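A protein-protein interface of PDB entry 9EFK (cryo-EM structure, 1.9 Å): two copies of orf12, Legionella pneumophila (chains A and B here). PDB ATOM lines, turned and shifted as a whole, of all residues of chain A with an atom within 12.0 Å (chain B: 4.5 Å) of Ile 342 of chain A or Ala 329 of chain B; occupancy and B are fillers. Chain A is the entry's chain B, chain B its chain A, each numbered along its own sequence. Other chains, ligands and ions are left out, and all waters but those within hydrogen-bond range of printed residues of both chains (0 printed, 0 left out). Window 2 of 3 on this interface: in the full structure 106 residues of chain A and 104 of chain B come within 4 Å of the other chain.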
ATOM      1  N   ALA A 329      18.154 -18.403 -31.979  1.00  0.00           N
ATOM      2  CA  ALA A 329      17.956 -17.774 -30.679  1.00  0.00           C
ATOM      3  C   ALA A 329      18.125 -18.767 -29.538  1.00  0.00           C
ATOM      4  O   ALA A 329      18.594 -18.390 -28.461  1.00  0.00           O
ATOM      5  CB  ALA A 329      16.581 -17.112 -30.614  1.00  0.00           C
ATOM      6  N   PHE A 330      17.733 -20.023 -29.735  1.00  0.00           N
ATOM      7  CA  PHE A 330      18.124 -21.082 -28.819  1.00  0.00           C
ATOM      8  C   PHE A 330      18.463 -22.336 -29.612  1.00  0.00           C
ATOM      9  O   PHE A 330      18.122 -22.467 -30.787  1.00  0.00           O
ATOM     10  CB  PHE A 330      17.057 -21.380 -27.751  1.00  0.00           C
ATOM     11  CG  PHE A 330      15.660 -21.552 -28.281  1.00  0.00           C
ATOM     12  CD1 PHE A 330      15.321 -22.636 -29.068  1.00  0.00           C
ATOM     13  CD2 PHE A 330      14.671 -20.651 -27.938  1.00  0.00           C
ATOM     14  CE1 PHE A 330      14.035 -22.793 -29.531  1.00  0.00           C
ATOM     15  CE2 PHE A 330      13.382 -20.811 -28.393  1.00  0.00           C
ATOM     16  CZ  PHE A 330      13.065 -21.883 -29.189  1.00  0.00           C
ATOM     17  N   ASN A 331      19.164 -23.249 -28.952  1.00  0.00           N
ATOM     18  CA  ASN A 331      19.643 -24.481 -29.568  1.00  0.00           C
ATOM     19  C   ASN A 331      18.531 -25.520 -29.509  1.00  0.00           C
ATOM     20  O   ASN A 331      18.243 -26.064 -28.441  1.00  0.00           O
ATOM     21  CB  ASN A 331      20.899 -24.965 -28.848  1.00  0.00           C
ATOM     22  CG  ASN A 331      21.605 -26.083 -29.576  1.00  0.00           C
ATOM     23  OD1 ASN A 331      20.997 -26.842 -30.319  1.00  0.00           O
ATOM     24  ND2 ASN A 331      22.901 -26.195 -29.354  1.00  0.00           N
ATOM     25  N   GLN A 332      17.917 -25.810 -30.659  1.00  0.00           N
ATOM     26  CA  GLN A 332      16.825 -26.777 -30.692  1.00  0.00           C
ATOM     27  C   GLN A 332      17.292 -28.176 -30.321  1.00  0.00           C
ATOM     28  O   GLN A 332      16.493 -28.987 -29.848  1.00  0.00           O
ATOM     29  CB  GLN A 332      16.170 -26.807 -32.073  1.00  0.00           C
ATOM     30  CG  GLN A 332      15.296 -25.615 -32.397  1.00  0.00           C
ATOM     31  CD  GLN A 332      16.085 -24.428 -32.891  1.00  0.00           C
ATOM     32  OE1 GLN A 332      17.252 -24.550 -33.248  1.00  0.00           O
ATOM     33  NE2 GLN A 332      15.451 -23.269 -32.916  1.00  0.00           N
ATOM     34  N   GLN A 333      18.568 -28.484 -30.545  1.00  0.00           N
ATOM     35  CA  GLN A 333      19.069 -29.826 -30.281  1.00  0.00           C
ATOM     36  C   GLN A 333      19.285 -30.089 -28.799  1.00  0.00           C
ATOM     37  O   GLN A 333      19.172 -31.238 -28.363  1.00  0.00           O
ATOM     38  CB  GLN A 333      20.372 -30.061 -31.041  1.00  0.00           C
ATOM     39  CG  GLN A 333      20.282 -29.761 -32.514  1.00  0.00           C
ATOM     40  CD  GLN A 333      19.213 -30.564 -33.198  1.00  0.00           C
ATOM     41  OE1 GLN A 333      19.113 -31.772 -33.005  1.00  0.00           O
ATOM     42  NE2 GLN A 333      18.395 -29.896 -33.999  1.00  0.00           N
ATOM     43  N   THR A 334      19.615 -29.065 -28.016  1.00  0.00           N
ATOM     44  CA  THR A 334      19.813 -29.231 -26.583  1.00  0.00           C
ATOM     45  C   THR A 334      18.667 -28.657 -25.762  1.00  0.00           C
ATOM     46  O   THR A 334      18.755 -28.632 -24.534  1.00  0.00           O
ATOM     47  CB  THR A 334      21.136 -28.600 -26.148  1.00  0.00           C
ATOM     48  OG1 THR A 334      21.055 -27.177 -26.269  1.00  0.00           O
ATOM     49  CG2 THR A 334      22.277 -29.109 -27.007  1.00  0.00           C
ATOM     50  N   PHE A 335      17.600 -28.196 -26.409  1.00  0.00           N
ATOM     51  CA  PHE A 335      16.436 -27.683 -25.697  1.00  0.00           C
ATOM     52  C   PHE A 335      15.887 -28.745 -24.753  1.00  0.00           C
ATOM     53  O   PHE A 335      15.651 -29.886 -25.155  1.00  0.00           O
ATOM     54  CB  PHE A 335      15.372 -27.257 -26.706  1.00  0.00           C
ATOM     55  CG  PHE A 335      14.251 -26.453 -26.121  1.00  0.00           C
ATOM     56  CD1 PHE A 335      13.159 -27.073 -25.549  1.00  0.00           C
ATOM     57  CD2 PHE A 335      14.276 -25.073 -26.172  1.00  0.00           C
ATOM     58  CE1 PHE A 335      12.125 -26.333 -25.019  1.00  0.00           C
ATOM     59  CE2 PHE A 335      13.244 -24.329 -25.646  1.00  0.00           C
ATOM     60  CZ  PHE A 335      12.167 -24.960 -25.067  1.00  0.00           C
ATOM     61  N   THR A 336      15.682 -28.366 -23.495  1.00  0.00           N
ATOM     62  CA  THR A 336      15.305 -29.305 -22.437  1.00  0.00           C
ATOM     63  C   THR A 336      13.975 -28.891 -21.825  1.00  0.00           C
ATOM     64  O   THR A 336      13.944 -28.035 -20.923  1.00  0.00           O
ATOM     65  CB  THR A 336      16.392 -29.365 -21.364  1.00  0.00           C
ATOM     66  OG1 THR A 336      17.643 -29.709 -21.967  1.00  0.00           O
ATOM     67  CG2 THR A 336      16.048 -30.395 -20.312  1.00  0.00           C
ATOM     68  N   PRO A 337      12.855 -29.448 -22.280  1.00  0.00           N
ATOM     69  CA  PRO A 337      11.526 -29.065 -21.755  1.00  0.00           C
ATOM     70  C   PRO A 337      11.058 -29.855 -20.530  1.00  0.00           C
ATOM     71  O   PRO A 337      10.223 -30.750 -20.594  1.00  0.00           O
ATOM     72  CB  PRO A 337      10.616 -29.313 -22.958  1.00  0.00           C
ATOM     73  CG  PRO A 337      11.264 -30.438 -23.676  1.00  0.00           C
ATOM     74  CD  PRO A 337      12.748 -30.345 -23.442  1.00  0.00           C
ATOM     75  N   ARG A 338      11.602 -29.507 -19.373  1.00  0.00           N
ATOM     76  CA  ARG A 338      11.272 -30.133 -18.104  1.00  0.00           C
ATOM     77  C   ARG A 338      10.931 -29.053 -17.092  1.00  0.00           C
ATOM     78  O   ARG A 338      11.367 -27.906 -17.232  1.00  0.00           O
ATOM     79  CB  ARG A 338      12.435 -30.985 -17.572  1.00  0.00           C
ATOM     80  CG  ARG A 338      13.171 -31.808 -18.612  1.00  0.00           C
ATOM     81  CD  ARG A 338      12.286 -32.817 -19.325  1.00  0.00           C
ATOM     82  NE  ARG A 338      11.738 -33.827 -18.428  1.00  0.00           N
ATOM     83  CZ  ARG A 338      10.449 -33.960 -18.148  1.00  0.00           C
ATOM     84  NH1 ARG A 338       9.536 -33.178 -18.699  1.00  0.00           N
ATOM     85  NH2 ARG A 338      10.067 -34.906 -17.297  1.00  0.00           N
ATOM     86  N   PRO A 339      10.138 -29.374 -16.072  1.00  0.00           N
ATOM     87  CA  PRO A 339       9.833 -28.371 -15.045  1.00  0.00           C
ATOM     88  C   PRO A 339      11.093 -27.912 -14.326  1.00  0.00           C
ATOM     89  O   PRO A 339      11.939 -28.718 -13.937  1.00  0.00           O
ATOM     90  CB  PRO A 339       8.871 -29.106 -14.105  1.00  0.00           C
ATOM     91  CG  PRO A 339       9.080 -30.545 -14.385  1.00  0.00           C
ATOM     92  CD  PRO A 339       9.426 -30.637 -15.826  1.00  0.00           C
ATOM     93  N   GLY A 340      11.213 -26.601 -14.158  1.00  0.00           N
ATOM     94  CA  GLY A 340      12.361 -25.994 -13.528  1.00  0.00           C
ATOM     95  C   GLY A 340      13.550 -25.765 -14.432  1.00  0.00           C
ATOM     96  O   GLY A 340      14.558 -25.224 -13.969  1.00  0.00           O
ATOM     97  N   SER A 341      13.465 -26.138 -15.702  1.00  0.00           N
ATOM     98  CA  SER A 341      14.606 -26.045 -16.599  1.00  0.00           C
ATOM     99  C   SER A 341      14.850 -24.609 -17.042  1.00  0.00           C
ATOM    100  O   SER A 341      13.912 -23.861 -17.323  1.00  0.00           O
ATOM    101  CB  SER A 341      14.385 -26.928 -17.824  1.00  0.00           C
ATOM    102  OG  SER A 341      15.399 -26.724 -18.784  1.00  0.00           O
ATOM    103  N   ILE A 342      16.122 -24.231 -17.112  1.00  0.00           N
ATOM    104  CA  ILE A 342      16.536 -22.962 -17.697  1.00  0.00           C
ATOM    105  C   ILE A 342      17.020 -23.228 -19.112  1.00  0.00           C
ATOM    106  O   ILE A 342      17.909 -24.056 -19.326  1.00  0.00           O
ATOM    107  CB  ILE A 342      17.647 -22.291 -16.875  1.00  0.00           C
ATOM    108  CG1 ILE A 342      17.241 -22.125 -15.416  1.00  0.00           C
ATOM    109  CG2 ILE A 342      17.999 -20.947 -17.477  1.00  0.00           C
ATOM    110  CD1 ILE A 342      18.374 -21.628 -14.556  1.00  0.00           C
ATOM    111  N   VAL A 343      16.441 -22.527 -20.075  1.00  0.00           N
ATOM    112  CA  VAL A 343      16.845 -22.625 -21.473  1.00  0.00           C
ATOM    113  C   VAL A 343      17.723 -21.422 -21.790  1.00  0.00           C
ATOM    114  O   VAL A 343      17.285 -20.283 -21.581  1.00  0.00           O
ATOM    115  CB  VAL A 343      15.634 -22.681 -22.412  1.00  0.00           C
ATOM    116  CG1 VAL A 343      16.097 -22.783 -23.853  1.00  0.00           C
ATOM    117  CG2 VAL A 343      14.764 -23.851 -22.051  1.00  0.00           C
ATOM    118  N   PRO A 344      18.953 -21.618 -22.260  1.00  0.00           N
ATOM    119  CA  PRO A 344      19.755 -20.480 -22.730  1.00  0.00           C
ATOM    120  C   PRO A 344      19.123 -19.892 -23.982  1.00  0.00           C
ATOM    121  O   PRO A 344      18.920 -20.591 -24.974  1.00  0.00           O
ATOM    122  CB  PRO A 344      21.124 -21.104 -23.021  1.00  0.00           C
ATOM    123  CG  PRO A 344      21.109 -22.419 -22.325  1.00  0.00           C
ATOM    124  CD  PRO A 344      19.699 -22.879 -22.336  1.00  0.00           C
ATOM    125  N   VAL A 345      18.779 -18.610 -23.921  1.00  0.00           N
ATOM    126  CA  VAL A 345      18.100 -17.929 -25.017  1.00  0.00           C
ATOM    127  C   VAL A 345      18.775 -16.587 -25.249  1.00  0.00           C
ATOM    128  O   VAL A 345      18.995 -15.827 -24.302  1.00  0.00           O
ATOM    129  CB  VAL A 345      16.600 -17.727 -24.729  1.00  0.00           C
ATOM    130  CG1 VAL A 345      15.945 -16.979 -25.862  1.00  0.00           C
ATOM    131  CG2 VAL A 345      15.915 -19.055 -24.508  1.00  0.00           C
ATOM    132  N   GLN A 346      19.096 -16.289 -26.503  1.00  0.00           N
ATOM    133  CA  GLN A 346      19.506 -14.940 -26.881  1.00  0.00           C
ATOM    134  C   GLN A 346      18.250 -14.085 -26.907  1.00  0.00           C
ATOM    135  O   GLN A 346      17.523 -14.057 -27.899  1.00  0.00           O
ATOM    136  CB  GLN A 346      20.212 -14.937 -28.229  1.00  0.00           C
ATOM    137  CG  GLN A 346      21.370 -15.895 -28.318  1.00  0.00           C
ATOM    138  CD  GLN A 346      22.137 -15.749 -29.610  1.00  0.00           C
ATOM    139  OE1 GLN A 346      22.727 -14.708 -29.874  1.00  0.00           O
ATOM    140  NE2 GLN A 346      22.126 -16.789 -30.426  1.00  0.00           N
ATOM    141  N   MET A 347      17.983 -13.394 -25.800  1.00  0.00           N
ATOM    142  CA  MET A 347      16.702 -12.721 -25.633  1.00  0.00           C
ATOM    143  C   MET A 347      16.552 -11.507 -26.539  1.00  0.00           C
ATOM    144  O   MET A 347      15.422 -11.134 -26.861  1.00  0.00           O
ATOM    145  CB  MET A 347      16.513 -12.340 -24.166  1.00  0.00           C
ATOM    146  CG  MET A 347      16.183 -13.541 -23.288  1.00  0.00           C
ATOM    147  SD  MET A 347      16.431 -13.290 -21.525  1.00  0.00           S
ATOM    148  CE  MET A 347      15.787 -11.635 -21.343  1.00  0.00           C
ATOM    149  N   TYR B 322      12.236 -21.381 -17.618  1.00  0.00           N
ATOM    150  CA  TYR B 322      12.832 -20.061 -17.539  1.00  0.00           C
ATOM    151  C   TYR B 322      13.776 -19.843 -18.707  1.00  0.00           C
ATOM    152  O   TYR B 322      14.332 -20.790 -19.263  1.00  0.00           O
ATOM    153  CB  TYR B 322      13.571 -19.875 -16.212  1.00  0.00           C
ATOM    154  CG  TYR B 322      12.667 -20.115 -15.033  1.00  0.00           C
ATOM    155  CD1 TYR B 322      11.880 -19.098 -14.521  1.00  0.00           C
ATOM    156  CD2 TYR B 322      12.569 -21.370 -14.459  1.00  0.00           C
ATOM    157  CE1 TYR B 322      11.037 -19.320 -13.462  1.00  0.00           C
ATOM    158  CE2 TYR B 322      11.730 -21.600 -13.400  1.00  0.00           C
ATOM    159  CZ  TYR B 322      10.966 -20.573 -12.906  1.00  0.00           C
ATOM    160  OH  TYR B 322      10.129 -20.803 -11.847  1.00  0.00           O
ATOM    161  N   ALA B 324      17.228 -17.598 -19.719  1.00  0.00           N
ATOM    162  CA  ALA B 324      18.334 -16.817 -19.196  1.00  0.00           C
ATOM    163  C   ALA B 324      19.471 -16.881 -20.199  1.00  0.00           C
ATOM    164  O   ALA B 324      19.414 -17.618 -21.182  1.00  0.00           O
ATOM    165  CB  ALA B 324      18.781 -17.322 -17.822  1.00  0.00           C
ATOM    166  N   SER B 326      22.258 -18.188 -19.446  1.00  0.00           N
ATOM    167  CA  SER B 326      22.872 -19.484 -19.211  1.00  0.00           C
ATOM    168  C   SER B 326      22.058 -20.243 -18.179  1.00  0.00           C
ATOM    169  O   SER B 326      21.408 -19.642 -17.324  1.00  0.00           O
ATOM    170  CB  SER B 326      24.323 -19.331 -18.740  1.00  0.00           C
ATOM    171  OG  SER B 326      24.835 -20.552 -18.240  1.00  0.00           O
ATOM    172  N   ASP B 327      22.110 -21.570 -18.257  1.00  0.00           N
ATOM    173  CA  ASP B 327      21.477 -22.398 -17.239  1.00  0.00           C
ATOM    174  C   ASP B 327      22.242 -22.402 -15.926  1.00  0.00           C
ATOM    175  O   ASP B 327      21.787 -23.029 -14.967  1.00  0.00           O
ATOM    176  CB  ASP B 327      21.294 -23.832 -17.743  1.00  0.00           C
ATOM    177  CG  ASP B 327      22.604 -24.510 -18.096  1.00  0.00           C
ATOM    178  OD1 ASP B 327      23.406 -23.928 -18.850  1.00  0.00           O
ATOM    179  OD2 ASP B 327      22.828 -25.641 -17.625  1.00  0.00           O
ATOM    180  N   SER B 328      23.383 -21.729 -15.857  1.00  0.00           N
ATOM    181  CA  SER B 328      24.106 -21.547 -14.609  1.00  0.00           C
ATOM    182  C   SER B 328      23.516 -20.445 -13.739  1.00  0.00           C
ATOM    183  O   SER B 328      24.152 -20.054 -12.759  1.00  0.00           O
ATOM    184  CB  SER B 328      25.573 -21.240 -14.894  1.00  0.00           C
ATOM    185  OG  SER B 328      25.713 -19.983 -15.521  1.00  0.00           O
ATOM    186  N   ALA B 329      22.324 -19.941 -14.072  1.00  0.00           N
ATOM    187  CA  ALA B 329      21.709 -18.901 -13.256  1.00  0.00           C
ATOM    188  C   ALA B 329      21.458 -19.379 -11.834  1.00  0.00           C
ATOM    189  O   ALA B 329      21.542 -18.586 -10.894  1.00  0.00           O
ATOM    190  CB  ALA B 329      20.410 -18.422 -13.895  1.00  0.00           C
ATOM    191  N   PHE B 330      21.137 -20.656 -11.651  1.00  0.00           N
ATOM    192  CA  PHE B 330      21.191 -21.256 -10.329  1.00  0.00           C
ATOM    193  C   PHE B 330      21.770 -22.658 -10.442  1.00  0.00           C
ATOM    194  O   PHE B 330      21.888 -23.222 -11.529  1.00  0.00           O
ATOM    195  CB  PHE B 330      19.825 -21.264  -9.620  1.00  0.00           C
ATOM    196  CG  PHE B 330      18.685 -21.796 -10.443  1.00  0.00           C
ATOM    197  CD1 PHE B 330      18.618 -23.130 -10.798  1.00  0.00           C
ATOM    198  CD2 PHE B 330      17.643 -20.963 -10.802  1.00  0.00           C
ATOM    199  CE1 PHE B 330      17.556 -23.610 -11.533  1.00  0.00           C
ATOM    200  CE2 PHE B 330      16.578 -21.438 -11.531  1.00  0.00           C
ATOM    201  CZ  PHE B 330      16.533 -22.764 -11.896  1.00  0.00           C
ATOM    202  N   GLN B 332      21.601 -26.398 -10.174  1.00  0.00           N
ATOM    203  CA  GLN B 332      20.577 -27.439 -10.186  1.00  0.00           C
ATOM    204  C   GLN B 332      20.853 -28.525  -9.154  1.00  0.00           C
ATOM    205  O   GLN B 332      19.918 -29.175  -8.679  1.00  0.00           O
ATOM    206  CB  GLN B 332      20.460 -28.067 -11.575  1.00  0.00           C
ATOM    207  CG  GLN B 332      19.770 -27.202 -12.611  1.00  0.00           C
ATOM    208  CD  GLN B 332      20.674 -26.137 -13.188  1.00  0.00           C
ATOM    209  OE1 GLN B 332      21.894 -26.218 -13.084  1.00  0.00           O
ATOM    210  NE2 GLN B 332      20.078 -25.129 -13.800  1.00  0.00           N
ATOM    211  N   PRO B 344      19.791 -19.319  -4.069  1.00  0.00           N
ATOM    212  CA  PRO B 344      20.727 -18.378  -4.702  1.00  0.00           C
ATOM    213  C   PRO B 344      20.541 -18.380  -6.210  1.00  0.00           C
ATOM    214  O   PRO B 344      20.638 -19.420  -6.860  1.00  0.00           O
ATOM    215  CB  PRO B 344      22.101 -18.922  -4.299  1.00  0.00           C
ATOM    216  CG  PRO B 344      21.846 -19.821  -3.150  1.00  0.00           C
ATOM    217  CD  PRO B 344      20.488 -20.386  -3.341  1.00  0.00           C
ATOM    218  N   VAL B 345      20.251 -17.206  -6.764  1.00  0.00           N
ATOM    219  CA  VAL B 345      19.974 -17.053  -8.188  1.00  0.00           C
ATOM    220  C   VAL B 345      20.707 -15.825  -8.703  1.00  0.00           C
ATOM    221  O   VAL B 345      20.666 -14.763  -8.075  1.00  0.00           O
ATOM    222  CB  VAL B 345      18.463 -16.926  -8.471  1.00  0.00           C
ATOM    223  CG1 VAL B 345      18.222 -16.664  -9.938  1.00  0.00           C
ATOM    224  CG2 VAL B 345      17.734 -18.177  -8.044  1.00  0.00           C
ATOM    225  N   GLN B 346      21.376 -15.962  -9.845  1.00  0.00           N
ATOM    226  CA  GLN B 346      21.928 -14.814 -10.559  1.00  0.00           C
ATOM    227  C   GLN B 346      20.783 -14.145 -11.301  1.00  0.00           C
ATOM    228  O   GLN B 346      20.427 -14.543 -12.409  1.00  0.00           O
ATOM    229  CB  GLN B 346      23.035 -15.243 -11.512  1.00  0.00           C
ATOM    230  CG  GLN B 346      24.154 -15.998 -10.844  1.00  0.00           C
ATOM    231  CD  GLN B 346      25.301 -16.276 -11.778  1.00  0.00           C
ATOM    232  OE1 GLN B 346      25.989 -15.363 -12.220  1.00  0.00           O
ATOM    233  NE2 GLN B 346      25.517 -17.542 -12.084  1.00  0.00           N
ATOM    234  N   GLN B 349      22.182 -11.625 -15.687  1.00  0.00           N
ATOM    235  CA  GLN B 349      23.433 -12.108 -16.271  1.00  0.00           C
ATOM    236  C   GLN B 349      23.721 -11.272 -17.514  1.00  0.00           C
ATOM    237  O   GLN B 349      23.088 -11.460 -18.556  1.00  0.00           O
ATOM    238  CB  GLN B 349      23.351 -13.593 -16.605  1.00  0.00           C
ATOM    239  CG  GLN B 349      23.409 -14.505 -15.403  1.00  0.00           C
ATOM    240  CD  GLN B 349      23.272 -15.961 -15.776  1.00  0.00           C
ATOM    241  OE1 GLN B 349      22.324 -16.354 -16.447  1.00  0.00           O
ATOM    242  NE2 GLN B 349      24.224 -16.772 -15.344  1.00  0.00           N
ATOM    243  N   ILE B 354      16.860 -13.226 -15.864  1.00  0.00           N
ATOM    244  CA  ILE B 354      16.150 -14.496 -15.932  1.00  0.00           C
ATOM    245  C   ILE B 354      14.662 -14.231 -15.754  1.00  0.00           C
ATOM    246  O   ILE B 354      14.252 -13.479 -14.864  1.00  0.00           O
ATOM    247  CB  ILE B 354      16.684 -15.483 -14.882  1.00  0.00           C
ATOM    248  CG1 ILE B 354      15.924 -16.807 -14.961  1.00  0.00           C
ATOM    249  CG2 ILE B 354      16.621 -14.891 -13.485  1.00  0.00           C
ATOM    250  CD1 ILE B 354      16.449 -17.866 -14.041  1.00  0.00           C
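Printed residues of chain B that touch a printed residue of chain A: Tyr 322, Ala 324, Ser 326, Asp 327, Ala 329, Phe 330 and Gln 332.
Hydrophobic or aromatic side chains of chain B that line the printed part of chain A: Ala 324, Ala 329 and Phe 330.
Hydrophobic or aromatic side chains of chain A within 4 Å of the printed part of chain B: Ile 342 and Val 343.
Along chain A the printed residues that touch a printed residue of chain B span positions 340 to 345.
The backbone NH (N) of Ala 324 of chain B lies within hydrogen-bond range of the backbone carbonyl oxygen (O) of Val 343 of chain A, 3.3 Å away.
N of Val 343 of chain A sits at hydrogen-bond distance from O of Tyr 322 of chain B.
The backbone carbonyl oxygen (O) of Ala 324 of chain B sits at hydrogen-bond distance from the backbone NH (N) of Val 345 of chain A, at 3.0 Å.
O of Ser 341 of chain A is in hydrogen-bond range of N of Tyr 322 of chain B (3.0 Å).
Gly 340 of chain A touches Phe 330 of chain B.
O of Tyr 322 of chain B touches CA of Ile 342 of chain A (3.5 Å).
Ala 324 of chain B touches Ile 342 of chain A (CB to CG2, 3.7 Å).
CG2 of Ile 342 of chain A touches O of Ser 326 of chain B (3.7 Å).
Asp 327 of chain B touches Ile 342 of chain A (O to CD1, 3.7 Å).
CD1 of Ile 342 of chain A touches CB of Ala 329 of chain B (3.9 Å).
CD1 of Ile 342 of chain A touches CZ of Phe 330 of chain B, 3.4 Å away.
Ile 342 of chain A touches Gln 332 of chain B.
Ala 324 of chain B touches Pro 344 of chain A.
Of the printed residues of chain B, Gly 340 of chain A touches Phe 330 (3.8 Å).
Of the printed residues of chain B, Ser 341 of chain A touches Tyr 322.
Ile 342 of chain A touches just these residues of chain B: Tyr 322 (3.5 Å), Ala 324 (3.7 Å), Ser 326 (3.7 Å), Asp 327 (3.7 Å), Ala 329 (3.9 Å), Phe 330 (3.4 Å) and Gln 332 (3.97 Å).
Of the printed residues of chain B, Pro 344 of chain A touches Ala 324.
Printed residues of chain B within 4 Å of Val 345 of chain A: Ala 324 (3.0 Å).
No residue of chain A comes within 4 Å of Ser 328 of chain B.
Of chain A, only Ile 342 (3.9 Å) comes within 4 Å of Ala 329 of chain B.
Phe 330 of chain B touches two residues of chain A.
Of the printed residues of chain A, Gln 332 of chain B touches Ile 342.
No residue of chain A comes within 4 Å of Pro 344 of chain B.
No residue of chain A comes within 4 Å of Gln 346 of chain B.
The nearest residue of chain B that does not touch Ile 342 of chain A is Ile 354 of chain B (4.3 Å).
6 positions are printed for both chains.
Of the 13 pairs that touch across the chains among the printed residues, none has its exchanged pair printed and touching as well.
The side-chain amide oxygen (OE1) of Gln 332 of chain B lies close to the backbone carbonyl oxygen (O) of Phe 330 of chain B (3.4 Å).
The side-chain hydroxyl of Ser 341 of chain A is in hydrogen-bond range of the backbone carbonyl oxygen of Thr 336 of chain A (2.9 Å).
The backbone NH of Gln 346 of chain B is in hydrogen-bond range of the backbone carbonyl oxygen of Ala 329 of chain B, at 2.8 Å.
The backbone carbonyl oxygen of Asp 327 of chain B lies within hydrogen-bond range of the side-chain amide nitrogen of Gln 332 of chain B, at 2.9 Å.
The side-chain hydroxyl (OG) of Ser 326 of chain B is in hydrogen-bond range of the side-chain hydroxyl (OG) of Ser 328 of chain B (2.9 Å).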
